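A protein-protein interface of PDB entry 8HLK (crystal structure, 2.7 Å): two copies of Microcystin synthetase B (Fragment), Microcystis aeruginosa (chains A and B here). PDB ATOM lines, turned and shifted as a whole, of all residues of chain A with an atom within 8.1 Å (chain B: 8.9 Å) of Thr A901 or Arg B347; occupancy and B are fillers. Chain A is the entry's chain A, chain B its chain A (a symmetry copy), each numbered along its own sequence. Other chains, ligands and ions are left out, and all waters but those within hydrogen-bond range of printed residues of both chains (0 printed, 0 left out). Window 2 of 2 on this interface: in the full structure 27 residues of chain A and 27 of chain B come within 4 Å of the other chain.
Among the printed residues, pairs that only touch across the chains: Thr A901 with Arg B347 (3.2 Å), Asp A903 with Leu B348 (3.99 Å), Asn A904 with Arg B347 (3.96 Å), Asn A904 with Pro B353 (3.8 Å), Arg A906 with Pro B353 (3.8 Å), Val A961 with Arg B347 (3.7 Å) and Asp A963 with Gly B354 (3.8 Å).
Thr A901 touches just one residue of chain B: Arg B347 (3.2 Å). Arg B347 touches just these residues of chain A: Asp A900 (3.1 Å), Thr A901 (3.2 Å), Asp A903 (2.7 Å), Asn A904 (3.96 Å) and Val A961 (3.7 Å). Asp A900 touches one residue of chain B. No residue of chain B comes within 4 Å of Ser A902. No residue of chain A comes within 4 Å of Gln B346. Printed residues of chain B within 4 Å of Val A961: Arg B347 (3.7 Å). Printed residues of chain A within 4 Å of Pro B353: Asn A904 (3.8 Å) and Arg A906 (3.8 Å). Arg A898 touches none of the printed residues of chain B. The nearest residue of chain B that does not touch Thr A901 is Glu B344 (4.8 Å).
No position is printed for both chains. Of the 9 pairs that touch across the chains among the printed residues, none has its exchanged pair printed and touching as well.
Of the 13 printed residues of chain A, 7 touch a printed residue of chain B. Of the 24 printed residues of chain B, 4 touch a printed residue of chain A. Hydrophobic or aromatic side chains of chain B that line the printed part of chain A: Pro B353. Among the printed residues, 9 pairs touch across the chains. Among the printed residues, Asp or Glu carboxylates within 4 Å of a Lys or Arg side-chain nitrogen of the other chain: Asp A900 with Arg B347.
OD1 of Asp A903 is in hydrogen-bond range of ND2 of Asn A904 (3.1 Å). The side-chain hydroxyl of Thr A901 sits at hydrogen-bond distance from the side-chain carboxylate of Asp A903. The side-chain carboxylate of Asp A963 lies within salt-bridge range of the guanidinium group of Arg A906 (3.2 Å). The backbone carbonyl oxygen (O) of Thr A901 sits at hydrogen-bond distance from the guanidinium group (NE) of Arg A898 (3.2 Å). OD1 of Asp A900 lies within hydrogen-bond range of ND2 of Asn A904 (3.2 Å).
O of Arg B347 lies close to OD1 of Asp A903 (2.7 Å). The side-chain carboxylate of Asp A900 is in salt-bridge range of the guanidinium group of Arg B347, 3.1 Å away.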
ATOM      1  N   ARG A 898      28.835  26.899  -6.436  1.00  0.00           N
ATOM      2  CA  ARG A 898      28.879  26.074  -5.235  1.00  0.00           C
ATOM      3  C   ARG A 898      29.555  26.880  -4.137  1.00  0.00           C
ATOM      4  O   ARG A 898      30.700  27.304  -4.303  1.00  0.00           O
ATOM      5  CB  ARG A 898      29.625  24.765  -5.524  1.00  0.00           C
ATOM      6  CG  ARG A 898      30.457  24.191  -4.381  1.00  0.00           C
ATOM      7  CD  ARG A 898      31.787  23.636  -4.883  1.00  0.00           C
ATOM      8  NE  ARG A 898      31.588  22.590  -5.888  1.00  0.00           N
ATOM      9  CZ  ARG A 898      32.549  21.923  -6.532  1.00  0.00           C
ATOM     10  NH1 ARG A 898      33.825  22.157  -6.278  1.00  0.00           N
ATOM     11  NH2 ARG A 898      32.228  20.997  -7.422  1.00  0.00           N
ATOM     12  N   GLU A 899      28.841  27.098  -3.024  1.00  0.00           N
ATOM     13  CA  GLU A 899      29.502  27.531  -1.803  1.00  0.00           C
ATOM     14  C   GLU A 899      29.758  26.329  -0.882  1.00  0.00           C
ATOM     15  O   GLU A 899      30.572  26.402   0.035  1.00  0.00           O
ATOM     16  CB  GLU A 899      28.671  28.614  -1.137  1.00  0.00           C
ATOM     17  CG  GLU A 899      29.447  29.293  -0.047  1.00  0.00           C
ATOM     18  CD  GLU A 899      30.438  30.298  -0.572  1.00  0.00           C
ATOM     19  OE1 GLU A 899      29.986  31.247  -1.223  1.00  0.00           O
ATOM     20  OE2 GLU A 899      31.640  30.119  -0.320  1.00  0.00           O
ATOM     21  N   ASP A 900      29.096  25.202  -1.176  1.00  0.00           N
ATOM     22  CA  ASP A 900      29.273  23.943  -0.470  1.00  0.00           C
ATOM     23  C   ASP A 900      30.566  23.367  -1.081  1.00  0.00           C
ATOM     24  O   ASP A 900      31.299  24.100  -1.736  1.00  0.00           O
ATOM     25  CB  ASP A 900      28.126  23.007  -0.900  1.00  0.00           C
ATOM     26  CG  ASP A 900      26.959  22.848   0.120  1.00  0.00           C
ATOM     27  OD1 ASP A 900      26.045  22.029  -0.147  1.00  0.00           O
ATOM     28  OD2 ASP A 900      26.949  23.556   1.153  1.00  0.00           O
ATOM     29  N   THR A 901      30.995  22.165  -0.723  1.00  0.00           N
ATOM     30  CA  THR A 901      32.264  21.564  -1.139  1.00  0.00           C
ATOM     31  C   THR A 901      32.146  20.755  -2.437  1.00  0.00           C
ATOM     32  O   THR A 901      31.186  20.957  -3.175  1.00  0.00           O
ATOM     33  CB  THR A 901      32.681  20.531  -0.077  1.00  0.00           C
ATOM     34  OG1 THR A 901      31.984  19.318  -0.404  1.00  0.00           O
ATOM     35  CG2 THR A 901      32.403  20.948   1.356  1.00  0.00           C
ATOM     36  N   SER A 902      33.077  19.808  -2.691  1.00  0.00           N
ATOM     37  CA  SER A 902      33.206  19.153  -3.993  1.00  0.00           C
ATOM     38  C   SER A 902      32.217  18.038  -4.357  1.00  0.00           C
ATOM     39  O   SER A 902      32.320  17.446  -5.433  1.00  0.00           O
ATOM     40  CB  SER A 902      34.647  18.674  -4.105  1.00  0.00           C
ATOM     41  OG  SER A 902      34.797  17.327  -3.680  1.00  0.00           O
ATOM     42  N   ASP A 903      31.243  17.760  -3.480  1.00  0.00           N
ATOM     43  CA  ASP A 903      30.196  16.789  -3.781  1.00  0.00           C
ATOM     44  C   ASP A 903      29.018  17.163  -4.687  1.00  0.00           C
ATOM     45  O   ASP A 903      28.770  16.531  -5.721  1.00  0.00           O
ATOM     46  CB  ASP A 903      29.479  16.332  -2.503  1.00  0.00           C
ATOM     47  CG  ASP A 903      28.800  17.451  -1.728  1.00  0.00           C
ATOM     48  OD1 ASP A 903      27.562  17.571  -1.842  1.00  0.00           O
ATOM     49  OD2 ASP A 903      29.516  18.201  -1.034  1.00  0.00           O
ATOM     50  N   ASN A 904      28.312  18.228  -4.290  1.00  0.00           N
ATOM     51  CA  ASN A 904      27.230  18.802  -5.068  1.00  0.00           C
ATOM     52  C   ASN A 904      27.676  20.190  -5.505  1.00  0.00           C
ATOM     53  O   ASN A 904      28.755  20.634  -5.125  1.00  0.00           O
ATOM     54  CB  ASN A 904      25.916  18.858  -4.275  1.00  0.00           C
ATOM     55  CG  ASN A 904      25.877  19.930  -3.199  1.00  0.00           C
ATOM     56  OD1 ASN A 904      26.355  21.046  -3.397  1.00  0.00           O
ATOM     57  ND2 ASN A 904      25.294  19.606  -2.054  1.00  0.00           N
ATOM     58  N   GLN A 905      26.768  20.924  -6.155  1.00  0.00           N
ATOM     59  CA  GLN A 905      27.060  22.342  -6.495  1.00  0.00           C
ATOM     60  C   GLN A 905      26.025  23.225  -5.784  1.00  0.00           C
ATOM     61  O   GLN A 905      26.459  24.139  -5.074  1.00  0.00           O
ATOM     62  CB  GLN A 905      27.060  22.554  -8.009  1.00  0.00           C
ATOM     63  CG  GLN A 905      28.458  22.704  -8.586  1.00  0.00           C
ATOM     64  CD  GLN A 905      28.700  21.778  -9.752  1.00  0.00           C
ATOM     65  OE1 GLN A 905      27.773  21.380 -10.454  1.00  0.00           O
ATOM     66  NE2 GLN A 905      29.956  21.428  -9.969  1.00  0.00           N
ATOM     67  N   ARG A 906      24.726  22.923  -5.919  1.00  0.00           N
ATOM     68  CA  ARG A 906      23.614  23.719  -5.302  1.00  0.00           C
ATOM     69  C   ARG A 906      23.696  25.254  -5.380  1.00  0.00           C
ATOM     70  O   ARG A 906      23.965  25.917  -4.357  1.00  0.00           O
ATOM     71  CB  ARG A 906      23.282  23.256  -3.870  1.00  0.00           C
ATOM     72  CG  ARG A 906      24.383  23.386  -2.826  1.00  0.00           C
ATOM     73  CD  ARG A 906      24.049  24.331  -1.686  1.00  0.00           C
ATOM     74  NE  ARG A 906      22.635  24.667  -1.613  1.00  0.00           N
ATOM     75  CZ  ARG A 906      21.914  24.631  -0.498  1.00  0.00           C
ATOM     76  NH1 ARG A 906      22.514  24.582   0.678  1.00  0.00           N
ATOM     77  NH2 ARG A 906      20.594  24.641  -0.564  1.00  0.00           N
ATOM     78  N   PRO A 960      29.229  33.056   3.687  1.00  0.00           N
ATOM     79  CA  PRO A 960      28.598  32.008   4.492  1.00  0.00           C
ATOM     80  C   PRO A 960      27.975  30.892   3.676  1.00  0.00           C
ATOM     81  O   PRO A 960      27.191  31.175   2.784  1.00  0.00           O
ATOM     82  CB  PRO A 960      27.444  32.709   5.205  1.00  0.00           C
ATOM     83  CG  PRO A 960      27.859  34.157   5.242  1.00  0.00           C
ATOM     84  CD  PRO A 960      28.665  34.378   3.980  1.00  0.00           C
ATOM     85  N   VAL A 961      28.326  29.643   3.997  1.00  0.00           N
ATOM     86  CA  VAL A 961      27.761  28.482   3.319  1.00  0.00           C
ATOM     87  C   VAL A 961      26.372  28.237   3.890  1.00  0.00           C
ATOM     88  O   VAL A 961      26.187  28.424   5.080  1.00  0.00           O
ATOM     89  CB  VAL A 961      28.647  27.240   3.479  1.00  0.00           C
ATOM     90  CG1 VAL A 961      28.100  26.084   2.678  1.00  0.00           C
ATOM     91  CG2 VAL A 961      30.095  27.502   3.082  1.00  0.00           C
ATOM     92  N   PRO A 962      25.331  27.942   3.075  1.00  0.00           N
ATOM     93  CA  PRO A 962      23.957  27.958   3.588  1.00  0.00           C
ATOM     94  C   PRO A 962      23.574  26.705   4.380  1.00  0.00           C
ATOM     95  O   PRO A 962      24.178  25.646   4.188  1.00  0.00           O
ATOM     96  CB  PRO A 962      23.094  28.177   2.333  1.00  0.00           C
ATOM     97  CG  PRO A 962      23.948  27.692   1.162  1.00  0.00           C
ATOM     98  CD  PRO A 962      25.394  27.722   1.619  1.00  0.00           C
ATOM     99  N   ASP A 963      22.610  26.907   5.311  1.00  0.00           N
ATOM    100  CA  ASP A 963      21.955  25.912   6.162  1.00  0.00           C
ATOM    101  C   ASP A 963      22.777  25.677   7.446  1.00  0.00           C
ATOM    102  O   ASP A 963      24.006  25.451   7.353  1.00  0.00           O
ATOM    103  CB  ASP A 963      21.528  24.657   5.376  1.00  0.00           C
ATOM    104  CG  ASP A 963      20.364  24.874   4.402  1.00  0.00           C
ATOM    105  OD1 ASP A 963      19.285  25.327   4.849  1.00  0.00           O
ATOM    106  OD2 ASP A 963      20.526  24.581   3.196  1.00  0.00           O
ATOM    107  N   PRO B  20      37.458  24.439  10.814  1.00  0.00           N
ATOM    108  CA  PRO B  20      36.524  24.755   9.738  1.00  0.00           C
ATOM    109  C   PRO B  20      35.188  25.159  10.358  1.00  0.00           C
ATOM    110  O   PRO B  20      34.570  26.166  10.009  1.00  0.00           O
ATOM    111  CB  PRO B  20      36.437  23.439   8.934  1.00  0.00           C
ATOM    112  CG  PRO B  20      37.721  22.668   9.268  1.00  0.00           C
ATOM    113  CD  PRO B  20      38.082  23.110  10.679  1.00  0.00           C
ATOM    114  N   GLY B  24      33.271  28.787   9.581  1.00  0.00           N
ATOM    115  CA  GLY B  24      31.895  28.814   9.122  1.00  0.00           C
ATOM    116  C   GLY B  24      31.048  29.667  10.053  1.00  0.00           C
ATOM    117  O   GLY B  24      30.447  30.646   9.642  1.00  0.00           O
ATOM    118  N   GLU B 202      35.912  11.973   4.230  1.00  0.00           N
ATOM    119  CA  GLU B 202      34.916  12.308   3.230  1.00  0.00           C
ATOM    120  C   GLU B 202      34.597  11.067   2.405  1.00  0.00           C
ATOM    121  O   GLU B 202      33.466  10.892   1.972  1.00  0.00           O
ATOM    122  CB  GLU B 202      35.412  13.415   2.296  1.00  0.00           C
ATOM    123  CG  GLU B 202      35.454  14.808   2.908  1.00  0.00           C
ATOM    124  CD  GLU B 202      36.451  15.735   2.227  1.00  0.00           C
ATOM    125  OE1 GLU B 202      37.177  15.248   1.321  1.00  0.00           O
ATOM    126  OE2 GLU B 202      36.517  16.932   2.613  1.00  0.00           O
ATOM    127  N   TRP B 205      32.322   8.807   4.838  1.00  0.00           N
ATOM    128  CA  TRP B 205      30.945   9.290   4.897  1.00  0.00           C
ATOM    129  C   TRP B 205      30.242   9.121   3.549  1.00  0.00           C
ATOM    130  O   TRP B 205      29.037   8.891   3.516  1.00  0.00           O
ATOM    131  CB  TRP B 205      30.847  10.737   5.420  1.00  0.00           C
ATOM    132  CG  TRP B 205      31.163  10.825   6.888  1.00  0.00           C
ATOM    133  CD1 TRP B 205      32.230  11.419   7.486  1.00  0.00           C
ATOM    134  CD2 TRP B 205      30.436  10.166   7.936  1.00  0.00           C
ATOM    135  NE1 TRP B 205      32.223  11.169   8.824  1.00  0.00           N
ATOM    136  CE2 TRP B 205      31.136  10.404   9.130  1.00  0.00           C
ATOM    137  CE3 TRP B 205      29.271   9.401   7.971  1.00  0.00           C
ATOM    138  CZ2 TRP B 205      30.690   9.920  10.352  1.00  0.00           C
ATOM    139  CZ3 TRP B 205      28.827   8.930   9.180  1.00  0.00           C
ATOM    140  CH2 TRP B 205      29.541   9.169  10.346  1.00  0.00           C
ATOM    141  N   GLN B 206      30.970   9.204   2.431  1.00  0.00           N
ATOM    142  CA  GLN B 206      30.318   9.072   1.138  1.00  0.00           C
ATOM    143  C   GLN B 206      29.966   7.597   0.960  1.00  0.00           C
ATOM    144  O   GLN B 206      28.810   7.284   0.677  1.00  0.00           O
ATOM    145  CB  GLN B 206      31.156   9.716   0.024  1.00  0.00           C
ATOM    146  CG  GLN B 206      30.667   9.449  -1.399  1.00  0.00           C
ATOM    147  CD  GLN B 206      31.289   8.193  -1.983  1.00  0.00           C
ATOM    148  OE1 GLN B 206      32.508   8.006  -1.955  1.00  0.00           O
ATOM    149  NE2 GLN B 206      30.455   7.301  -2.504  1.00  0.00           N
ATOM    150  N   LEU B 209      27.030   6.329   3.416  1.00  0.00           N
ATOM    151  CA  LEU B 209      25.705   6.937   3.403  1.00  0.00           C
ATOM    152  C   LEU B 209      25.017   6.848   2.036  1.00  0.00           C
ATOM    153  O   LEU B 209      23.972   7.482   1.825  1.00  0.00           O
ATOM    154  CB  LEU B 209      25.827   8.390   3.872  1.00  0.00           C
ATOM    155  CG  LEU B 209      25.434   8.650   5.326  1.00  0.00           C
ATOM    156  CD1 LEU B 209      26.228   7.772   6.274  1.00  0.00           C
ATOM    157  CD2 LEU B 209      25.627  10.118   5.674  1.00  0.00           C
ATOM    158  N   VAL B 340      34.963  15.900  10.560  1.00  0.00           N
ATOM    159  CA  VAL B 340      34.298  16.698   9.542  1.00  0.00           C
ATOM    160  C   VAL B 340      32.906  17.020  10.075  1.00  0.00           C
ATOM    161  O   VAL B 340      32.257  16.150  10.647  1.00  0.00           O
ATOM    162  CB  VAL B 340      34.228  15.972   8.186  1.00  0.00           C
ATOM    163  CG1 VAL B 340      35.595  15.560   7.679  1.00  0.00           C
ATOM    164  CG2 VAL B 340      33.336  14.755   8.252  1.00  0.00           C
ATOM    165  N   SER B 341      32.466  18.269   9.907  1.00  0.00           N
ATOM    166  CA  SER B 341      31.236  18.716  10.520  1.00  0.00           C
ATOM    167  C   SER B 341      30.066  17.910   9.966  1.00  0.00           C
ATOM    168  O   SER B 341      30.174  17.169   8.993  1.00  0.00           O
ATOM    169  CB  SER B 341      31.010  20.211  10.350  1.00  0.00           C
ATOM    170  OG  SER B 341      30.315  20.536   9.144  1.00  0.00           O
ATOM    171  N   LEU B 342      28.938  18.070  10.643  1.00  0.00           N
ATOM    172  CA  LEU B 342      27.706  17.439  10.245  1.00  0.00           C
ATOM    173  C   LEU B 342      27.198  18.120   8.966  1.00  0.00           C
ATOM    174  O   LEU B 342      26.751  17.464   8.034  1.00  0.00           O
ATOM    175  CB  LEU B 342      26.780  17.580  11.461  1.00  0.00           C
ATOM    176  CG  LEU B 342      25.479  16.791  11.462  1.00  0.00           C
ATOM    177  CD1 LEU B 342      25.698  15.294  11.316  1.00  0.00           C
ATOM    178  CD2 LEU B 342      24.760  17.087  12.741  1.00  0.00           C
ATOM    179  N   ALA B 343      27.316  19.447   8.875  1.00  0.00           N
ATOM    180  CA  ALA B 343      26.988  20.141   7.634  1.00  0.00           C
ATOM    181  C   ALA B 343      27.841  19.598   6.489  1.00  0.00           C
ATOM    182  O   ALA B 343      27.355  19.394   5.385  1.00  0.00           O
ATOM    183  CB  ALA B 343      27.179  21.618   7.829  1.00  0.00           C
ATOM    184  N   GLU B 344      29.115  19.319   6.764  1.00  0.00           N
ATOM    185  CA  GLU B 344      29.972  18.698   5.773  1.00  0.00           C
ATOM    186  C   GLU B 344      29.450  17.297   5.470  1.00  0.00           C
ATOM    187  O   GLU B 344      29.522  16.854   4.337  1.00  0.00           O
ATOM    188  CB  GLU B 344      31.442  18.707   6.225  1.00  0.00           C
ATOM    189  CG  GLU B 344      32.154  20.056   6.032  1.00  0.00           C
ATOM    190  CD  GLU B 344      33.154  20.481   7.107  1.00  0.00           C
ATOM    191  OE1 GLU B 344      34.060  19.684   7.444  1.00  0.00           O
ATOM    192  OE2 GLU B 344      33.023  21.619   7.625  1.00  0.00           O
ATOM    193  N   ILE B 345      28.928  16.580   6.472  1.00  0.00           N
ATOM    194  CA  ILE B 345      28.481  15.212   6.241  1.00  0.00           C
ATOM    195  C   ILE B 345      27.138  15.237   5.506  1.00  0.00           C
ATOM    196  O   ILE B 345      26.920  14.396   4.646  1.00  0.00           O
ATOM    197  CB  ILE B 345      28.488  14.352   7.530  1.00  0.00           C
ATOM    198  CG1 ILE B 345      29.886  14.334   8.157  1.00  0.00           C
ATOM    199  CG2 ILE B 345      28.040  12.935   7.234  1.00  0.00           C
ATOM    200  CD1 ILE B 345      30.101  13.394   9.313  1.00  0.00           C
ATOM    201  N   GLN B 346      26.279  16.240   5.751  1.00  0.00           N
ATOM    202  CA  GLN B 346      24.977  16.284   5.097  1.00  0.00           C
ATOM    203  C   GLN B 346      25.193  16.366   3.600  1.00  0.00           C
ATOM    204  O   GLN B 346      24.772  15.484   2.853  1.00  0.00           O
ATOM    205  CB  GLN B 346      24.084  17.441   5.559  1.00  0.00           C
ATOM    206  CG  GLN B 346      22.655  17.395   5.005  1.00  0.00           C
ATOM    207  CD  GLN B 346      22.513  18.082   3.664  1.00  0.00           C
ATOM    208  OE1 GLN B 346      22.562  19.310   3.568  1.00  0.00           O
ATOM    209  NE2 GLN B 346      22.335  17.298   2.607  1.00  0.00           N
ATOM    210  N   ARG B 347      25.880  17.421   3.175  1.00  0.00           N
ATOM    211  CA  ARG B 347      26.060  17.658   1.753  1.00  0.00           C
ATOM    212  C   ARG B 347      26.752  16.460   1.095  1.00  0.00           C
ATOM    213  O   ARG B 347      26.339  16.009   0.031  1.00  0.00           O
ATOM    214  CB  ARG B 347      26.808  18.975   1.547  1.00  0.00           C
ATOM    215  CG  ARG B 347      28.195  19.002   2.159  1.00  0.00           C
ATOM    216  CD  ARG B 347      28.917  20.319   1.890  1.00  0.00           C
ATOM    217  NE  ARG B 347      28.521  21.439   2.739  1.00  0.00           N
ATOM    218  CZ  ARG B 347      29.265  21.967   3.721  1.00  0.00           C
ATOM    219  NH1 ARG B 347      30.520  21.579   3.921  1.00  0.00           N
ATOM    220  NH2 ARG B 347      28.736  22.902   4.497  1.00  0.00           N
ATOM    221  N   LEU B 348      27.734  15.887   1.788  1.00  0.00           N
ATOM    222  CA  LEU B 348      28.529  14.764   1.307  1.00  0.00           C
ATOM    223  C   LEU B 348      27.693  13.496   1.076  1.00  0.00           C
ATOM    224  O   LEU B 348      28.156  12.541   0.451  1.00  0.00           O
ATOM    225  CB  LEU B 348      29.611  14.565   2.375  1.00  0.00           C
ATOM    226  CG  LEU B 348      30.780  13.636   2.068  1.00  0.00           C
ATOM    227  CD1 LEU B 348      31.294  13.774   0.645  1.00  0.00           C
ATOM    228  CD2 LEU B 348      31.919  13.943   3.026  1.00  0.00           C
ATOM    229  N   SER B 349      26.458  13.486   1.594  1.00  0.00           N
ATOM    230  CA  SER B 349      25.550  12.352   1.491  1.00  0.00           C
ATOM    231  C   SER B 349      24.714  12.454   0.221  1.00  0.00           C
ATOM    232  O   SER B 349      24.839  13.436  -0.529  1.00  0.00           O
ATOM    233  CB  SER B 349      24.635  12.309   2.687  1.00  0.00           C
ATOM    234  OG  SER B 349      23.685  13.366   2.615  1.00  0.00           O
ATOM    235  N   ASP B 350      23.804  11.475   0.047  1.00  0.00           N
ATOM    236  CA  ASP B 350      22.853  11.534  -1.057  1.00  0.00           C
ATOM    237  C   ASP B 350      21.581  12.268  -0.644  1.00  0.00           C
ATOM    238  O   ASP B 350      20.656  12.342  -1.435  1.00  0.00           O
ATOM    239  CB  ASP B 350      22.574  10.156  -1.667  1.00  0.00           C
ATOM    240  CG  ASP B 350      23.630   9.724  -2.678  1.00  0.00           C
ATOM    241  OD1 ASP B 350      24.268   8.651  -2.471  1.00  0.00           O
ATOM    242  OD2 ASP B 350      23.828  10.479  -3.665  1.00  0.00           O
ATOM    243  N   ILE B 351      21.539  12.858   0.553  1.00  0.00           N
ATOM    244  CA  ILE B 351      20.330  13.542   0.969  1.00  0.00           C
ATOM    245  C   ILE B 351      20.299  14.854   0.197  1.00  0.00           C
ATOM    246  O   ILE B 351      21.324  15.517   0.084  1.00  0.00           O
ATOM    247  CB  ILE B 351      20.259  13.751   2.504  1.00  0.00           C
ATOM    248  CG1 ILE B 351      20.401  12.446   3.295  1.00  0.00           C
ATOM    249  CG2 ILE B 351      18.995  14.499   2.936  1.00  0.00           C
ATOM    250  CD1 ILE B 351      19.212  11.521   3.207  1.00  0.00           C
ATOM    251  N   PRO B 352      19.133  15.288  -0.325  1.00  0.00           N
ATOM    252  CA  PRO B 352      19.046  16.557  -1.024  1.00  0.00           C
ATOM    253  C   PRO B 352      19.546  17.665  -0.124  1.00  0.00           C
ATOM    254  O   PRO B 352      19.431  17.574   1.091  1.00  0.00           O
ATOM    255  CB  PRO B 352      17.554  16.806  -1.301  1.00  0.00           C
ATOM    256  CG  PRO B 352      16.842  15.811  -0.430  1.00  0.00           C
ATOM    257  CD  PRO B 352      17.810  14.650  -0.234  1.00  0.00           C
ATOM    258  N   PRO B 353      20.109  18.733  -0.727  1.00  0.00           N
ATOM    259  CA  PRO B 353      20.360  19.981  -0.021  1.00  0.00           C
ATOM    260  C   PRO B 353      19.060  20.527   0.534  1.00  0.00           C
ATOM    261  O   PRO B 353      18.025  20.405  -0.108  1.00  0.00           O
ATOM    262  CB  PRO B 353      20.906  20.916  -1.106  1.00  0.00           C
ATOM    263  CG  PRO B 353      21.481  19.990  -2.157  1.00  0.00           C
ATOM    264  CD  PRO B 353      20.568  18.781  -2.126  1.00  0.00           C
ATOM    265  N   GLY B 354      19.142  21.095   1.733  1.00  0.00           N
ATOM    266  CA  GLY B 354      18.024  21.800   2.332  1.00  0.00           C
ATOM    267  C   GLY B 354      17.355  20.985   3.436  1.00  0.00           C
ATOM    268  O   GLY B 354      16.796  21.581   4.362  1.00  0.00           O
ATOM    269  N   VAL B 355      17.417  19.639   3.323  1.00  0.00           N
ATOM    270  CA  VAL B 355      16.712  18.762   4.242  1.00  0.00           C
ATOM    271  C   VAL B 355      17.681  18.077   5.207  1.00  0.00           C
ATOM    272  O   VAL B 355      18.812  17.697   4.832  1.00  0.00           O
ATOM    273  CB  VAL B 355      15.871  17.705   3.504  1.00  0.00           C
ATOM    274  CG1 VAL B 355      15.016  18.342   2.424  1.00  0.00           C
ATOM    275  CG2 VAL B 355      16.707  16.549   2.966  1.00  0.00           C
ATOM    276  N   PRO B 356      17.193  17.820   6.453  1.00  0.00           N
ATOM    277  CA  PRO B 356      17.998  17.222   7.521  1.00  0.00           C
ATOM    278  C   PRO B 356      18.302  15.796   7.138  1.00  0.00           C
ATOM    279  O   PRO B 356      17.550  15.226   6.366  1.00  0.00           O
ATOM    280  CB  PRO B 356      17.082  17.203   8.746  1.00  0.00           C
ATOM    281  CG  PRO B 356      15.682  17.196   8.150  1.00  0.00           C
ATOM    282  CD  PRO B 356      15.795  18.013   6.882  1.00  0.00           C
ATOM    283  N   LEU B 357      19.377  15.210   7.646  1.00  0.00           N
ATOM    284  CA  LEU B 357      19.518  13.794   7.334  1.00  0.00           C
ATOM    285  C   LEU B 357      18.961  12.932   8.471  1.00  0.00           C
ATOM    286  O   LEU B 357      18.916  11.714   8.361  1.00  0.00           O
ATOM    287  CB  LEU B 357      20.941  13.423   6.917  1.00  0.00           C
ATOM    288  CG  LEU B 357      22.011  13.604   7.960  1.00  0.00           C
ATOM    289  CD1 LEU B 357      23.290  12.979   7.440  1.00  0.00           C
ATOM    290  CD2 LEU B 357      22.196  15.076   8.279  1.00  0.00           C
